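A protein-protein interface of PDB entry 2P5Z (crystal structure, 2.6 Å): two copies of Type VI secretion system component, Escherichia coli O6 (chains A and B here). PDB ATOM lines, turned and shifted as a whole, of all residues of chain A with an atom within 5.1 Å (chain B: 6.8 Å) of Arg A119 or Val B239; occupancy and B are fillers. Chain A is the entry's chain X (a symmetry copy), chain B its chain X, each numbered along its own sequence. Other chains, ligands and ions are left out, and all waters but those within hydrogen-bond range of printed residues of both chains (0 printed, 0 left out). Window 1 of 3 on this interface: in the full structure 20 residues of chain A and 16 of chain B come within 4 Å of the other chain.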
ATOM      1  N   LEU A  62      10.909  18.146  33.033  1.00  0.00           N
ATOM      2  CA  LEU A  62      12.042  18.878  32.434  1.00  0.00           C
ATOM      3  C   LEU A  62      12.925  19.525  33.474  1.00  0.00           C
ATOM      4  O   LEU A  62      12.433  20.138  34.409  1.00  0.00           O
ATOM      5  CB  LEU A  62      11.554  19.960  31.479  1.00  0.00           C
ATOM      6  CG  LEU A  62      10.935  19.444  30.181  1.00  0.00           C
ATOM      7  CD1 LEU A  62      10.310  20.611  29.391  1.00  0.00           C
ATOM      8  CD2 LEU A  62      11.985  18.655  29.371  1.00  0.00           C
ATOM      9  N   MET A  63      14.229  19.343  33.305  1.00  0.00           N
ATOM     10  CA  MET A  63      15.268  19.810  34.221  1.00  0.00           C
ATOM     11  C   MET A  63      15.353  19.072  35.576  1.00  0.00           C
ATOM     12  O   MET A  63      16.307  19.272  36.323  1.00  0.00           O
ATOM     13  CB  MET A  63      15.313  21.354  34.320  1.00  0.00           C
ATOM     14  CG  MET A  63      15.742  22.050  32.979  1.00  0.00           C
ATOM     15  SD  MET A  63      17.462  21.648  32.489  1.00  0.00           S
ATOM     16  CE  MET A  63      18.355  22.532  33.757  1.00  0.00           C
ATOM     17  N   THR A  92      16.189  16.247  29.746  1.00  0.00           N
ATOM     18  CA  THR A  92      16.369  17.307  28.762  1.00  0.00           C
ATOM     19  C   THR A  92      15.141  17.486  27.875  1.00  0.00           C
ATOM     20  O   THR A  92      14.833  18.584  27.429  1.00  0.00           O
ATOM     21  CB  THR A  92      17.584  16.947  27.926  1.00  0.00           C
ATOM     22  OG1 THR A  92      18.746  17.424  28.609  1.00  0.00           O
ATOM     23  CG2 THR A  92      17.515  17.518  26.530  1.00  0.00           C
ATOM     24  N   ALA A 115      25.955  18.064  29.397  1.00  0.00           N
ATOM     25  CA  ALA A 115      25.189  18.426  28.189  1.00  0.00           C
ATOM     26  C   ALA A 115      24.576  19.824  28.253  1.00  0.00           C
ATOM     27  O   ALA A 115      24.369  20.445  27.222  1.00  0.00           O
ATOM     28  CB  ALA A 115      24.102  17.429  27.919  1.00  0.00           C
ATOM     29  N   LEU A 116      24.300  20.322  29.455  1.00  0.00           N
ATOM     30  CA  LEU A 116      23.677  21.639  29.585  1.00  0.00           C
ATOM     31  C   LEU A 116      24.599  22.802  29.232  1.00  0.00           C
ATOM     32  O   LEU A 116      24.105  23.895  29.002  1.00  0.00           O
ATOM     33  CB  LEU A 116      23.085  21.850  30.971  1.00  0.00           C
ATOM     34  CG  LEU A 116      21.991  20.876  31.371  1.00  0.00           C
ATOM     35  CD1 LEU A 116      21.706  21.091  32.853  1.00  0.00           C
ATOM     36  CD2 LEU A 116      20.719  21.051  30.510  1.00  0.00           C
ATOM     37  N   LEU A 117      25.914  22.553  29.128  1.00  0.00           N
ATOM     38  CA  LEU A 117      26.870  23.554  28.626  1.00  0.00           C
ATOM     39  C   LEU A 117      26.572  24.029  27.204  1.00  0.00           C
ATOM     40  O   LEU A 117      27.158  24.997  26.738  1.00  0.00           O
ATOM     41  CB  LEU A 117      28.316  23.054  28.621  1.00  0.00           C
ATOM     42  CG  LEU A 117      29.111  22.400  29.749  1.00  0.00           C
ATOM     43  CD1 LEU A 117      30.535  22.914  29.727  1.00  0.00           C
ATOM     44  CD2 LEU A 117      28.472  22.499  31.140  1.00  0.00           C
ATOM     45  N   THR A 118      25.671  23.346  26.515  1.00  0.00           N
ATOM     46  CA  THR A 118      25.271  23.714  25.164  1.00  0.00           C
ATOM     47  C   THR A 118      24.296  24.885  25.239  1.00  0.00           C
ATOM     48  O   THR A 118      24.095  25.597  24.272  1.00  0.00           O
ATOM     49  CB  THR A 118      24.697  22.463  24.450  1.00  0.00           C
ATOM     50  OG1 THR A 118      25.783  21.558  24.212  1.00  0.00           O
ATOM     51  CG2 THR A 118      24.040  22.766  23.130  1.00  0.00           C
ATOM     52  N   ARG A 119      23.740  25.114  26.421  1.00  0.00           N
ATOM     53  CA  ARG A 119      22.743  26.151  26.594  1.00  0.00           C
ATOM     54  C   ARG A 119      23.295  27.561  26.838  1.00  0.00           C
ATOM     55  O   ARG A 119      22.530  28.517  26.854  1.00  0.00           O
ATOM     56  CB  ARG A 119      21.726  25.749  27.668  1.00  0.00           C
ATOM     57  CG  ARG A 119      20.410  25.223  27.088  1.00  0.00           C
ATOM     58  CD  ARG A 119      19.572  24.442  28.105  1.00  0.00           C
ATOM     59  NE  ARG A 119      19.568  25.003  29.464  1.00  0.00           N
ATOM     60  CZ  ARG A 119      18.719  25.933  29.903  1.00  0.00           C
ATOM     61  NH1 ARG A 119      17.802  26.449  29.090  1.00  0.00           N
ATOM     62  NH2 ARG A 119      18.800  26.359  31.158  1.00  0.00           N
ATOM     63  N   SER A 120      24.610  27.698  26.993  1.00  0.00           N
ATOM     64  CA  SER A 120      25.209  29.015  27.201  1.00  0.00           C
ATOM     65  C   SER A 120      26.340  29.311  26.232  1.00  0.00           C
ATOM     66  O   SER A 120      27.287  28.520  26.126  1.00  0.00           O
ATOM     67  CB  SER A 120      25.685  29.198  28.645  1.00  0.00           C
ATOM     68  OG  SER A 120      26.917  28.550  28.875  1.00  0.00           O
ATOM     69  N   ARG A 121      26.234  30.447  25.540  1.00  0.00           N
ATOM     70  CA  ARG A 121      27.200  30.829  24.505  1.00  0.00           C
ATOM     71  C   ARG A 121      27.687  32.278  24.603  1.00  0.00           C
ATOM     72  O   ARG A 121      27.372  33.118  23.759  1.00  0.00           O
ATOM     73  CB  ARG A 121      26.677  30.528  23.082  1.00  0.00           C
ATOM     74  CG  ARG A 121      25.262  31.026  22.731  1.00  0.00           C
ATOM     75  CD  ARG A 121      24.781  30.538  21.336  1.00  0.00           C
ATOM     76  NE  ARG A 121      25.846  30.449  20.325  1.00  0.00           N
ATOM     77  CZ  ARG A 121      26.244  29.312  19.740  1.00  0.00           C
ATOM     78  NH1 ARG A 121      25.672  28.156  20.059  1.00  0.00           N
ATOM     79  NH2 ARG A 121      27.214  29.322  18.832  1.00  0.00           N
ATOM     80  N   ARG A 142      30.056  29.200  35.363  1.00  0.00           N
ATOM     81  CA  ARG A 142      28.758  29.242  34.701  1.00  0.00           C
ATOM     82  C   ARG A 142      27.857  28.017  35.006  1.00  0.00           C
ATOM     83  O   ARG A 142      26.647  28.059  34.823  1.00  0.00           O
ATOM     84  CB  ARG A 142      28.995  29.431  33.195  1.00  0.00           C
ATOM     85  CG  ARG A 142      27.753  29.578  32.322  1.00  0.00           C
ATOM     86  CD  ARG A 142      26.883  30.777  32.685  1.00  0.00           C
ATOM     87  NE  ARG A 142      25.754  30.856  31.760  1.00  0.00           N
ATOM     88  CZ  ARG A 142      24.473  30.743  32.100  1.00  0.00           C
ATOM     89  NH1 ARG A 142      24.118  30.574  33.371  1.00  0.00           N
ATOM     90  NH2 ARG A 142      23.542  30.815  31.157  1.00  0.00           N
ATOM     91  N   TYR B 237       8.735  18.505  24.046  1.00  0.00           N
ATOM     92  CA  TYR B 237       9.177  19.682  24.769  1.00  0.00           C
ATOM     93  C   TYR B 237      10.626  19.480  25.027  1.00  0.00           C
ATOM     94  O   TYR B 237      11.059  18.383  25.379  1.00  0.00           O
ATOM     95  CB  TYR B 237       8.459  19.836  26.098  1.00  0.00           C
ATOM     96  CG  TYR B 237       6.999  20.189  25.998  1.00  0.00           C
ATOM     97  CD1 TYR B 237       6.023  19.198  25.842  1.00  0.00           C
ATOM     98  CD2 TYR B 237       6.579  21.501  26.117  1.00  0.00           C
ATOM     99  CE1 TYR B 237       4.673  19.526  25.773  1.00  0.00           C
ATOM    100  CE2 TYR B 237       5.228  21.828  26.060  1.00  0.00           C
ATOM    101  CZ  TYR B 237       4.290  20.839  25.878  1.00  0.00           C
ATOM    102  OH  TYR B 237       2.960  21.174  25.811  1.00  0.00           O
ATOM    103  N   SER B 238      11.396  20.536  24.832  1.00  0.00           N
ATOM    104  CA  SER B 238      12.833  20.406  24.893  1.00  0.00           C
ATOM    105  C   SER B 238      13.392  21.475  25.795  1.00  0.00           C
ATOM    106  O   SER B 238      12.659  22.344  26.271  1.00  0.00           O
ATOM    107  CB  SER B 238      13.428  20.520  23.492  1.00  0.00           C
ATOM    108  OG  SER B 238      14.636  19.784  23.420  1.00  0.00           O
ATOM    109  N   VAL B 239      14.699  21.407  26.009  1.00  0.00           N
ATOM    110  CA  VAL B 239      15.416  22.336  26.869  1.00  0.00           C
ATOM    111  C   VAL B 239      16.867  22.459  26.387  1.00  0.00           C
ATOM    112  O   VAL B 239      17.334  21.664  25.559  1.00  0.00           O
ATOM    113  CB  VAL B 239      15.372  21.861  28.338  1.00  0.00           C
ATOM    114  CG1 VAL B 239      16.757  21.823  28.932  1.00  0.00           C
ATOM    115  CG2 VAL B 239      14.415  22.729  29.154  1.00  0.00           C
ATOM    116  N   GLU B 309      10.280  26.842  19.515  1.00  0.00           N
ATOM    117  CA  GLU B 309      10.916  25.537  19.363  1.00  0.00           C
ATOM    118  C   GLU B 309      10.987  24.742  20.670  1.00  0.00           C
ATOM    119  O   GLU B 309      11.541  23.657  20.707  1.00  0.00           O
ATOM    120  CB  GLU B 309      12.301  25.694  18.740  1.00  0.00           C
ATOM    121  CG  GLU B 309      13.164  26.710  19.448  1.00  0.00           C
ATOM    122  CD  GLU B 309      14.466  26.998  18.719  1.00  0.00           C
ATOM    123  OE1 GLU B 309      15.536  26.882  19.361  1.00  0.00           O
ATOM    124  OE2 GLU B 309      14.423  27.342  17.512  1.00  0.00           O
ATOM    125  N   GLN B 310      10.406  25.296  21.730  1.00  0.00           N
ATOM    126  CA  GLN B 310      10.383  24.672  23.047  1.00  0.00           C
ATOM    127  C   GLN B 310       9.222  23.685  23.175  1.00  0.00           C
ATOM    128  O   GLN B 310       9.242  22.804  24.028  1.00  0.00           O
ATOM    129  CB  GLN B 310      10.208  25.749  24.118  1.00  0.00           C
ATOM    130  CG  GLN B 310      10.783  25.389  25.477  1.00  0.00           C
ATOM    131  CD  GLN B 310      10.325  26.323  26.577  1.00  0.00           C
ATOM    132  OE1 GLN B 310      10.943  26.391  27.640  1.00  0.00           O
ATOM    133  NE2 GLN B 310       9.232  27.044  26.334  1.00  0.00           N
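O of Gln B310 is in hydrogen-bond range of N of Ser B238 (3.2 Å).
No position is printed for both chains.
Among the printed residues, pairs that only touch across the chains: Thr A92 with Ser B238, Met A63 with Val B239, Arg A119 with Val B239 and Leu A62 with Tyr B237.
The backbone NH (N) of Val B239 sits at hydrogen-bond distance from the backbone carbonyl oxygen (O) of Thr A92, 3.2 Å away.
Hydrophobic or aromatic side chains of chain A that line the printed part of chain B: Leu A62 and Met A63. Of the 5 printed residues of chain B, 3 touch a printed residue of chain A. Printed residues of chain B that touch a printed residue of chain A: Tyr B237, Ser B238 and Val B239. Hydrophobic or aromatic side chains of chain B that line the printed part of chain A: Tyr B237 and Val B239. Among the printed residues, no Asp or Glu carboxylate lies within 4 Å of a Lys or Arg side-chain nitrogen of the other chain.
Of the printed residues of chain B, Leu A62 touches Tyr B237. Of the printed residues of chain B, Met A63 touches Val B239 (3.6 Å). Arg A119 touches just one residue of chain B: Val B239 (3.8 Å). Arg A121 touches none of the printed residues of chain B. Val B239 touches just these residues of chain A: Met A63, Thr A92 and Arg A119. Gln B310 touches none of the printed residues of chain A. The nearest residue of chain A that does not touch Val B239 is Leu A116 (4.3 Å). The nearest printed residue of chain B that does not touch Met A63 is Ser B238 (7.4 Å).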
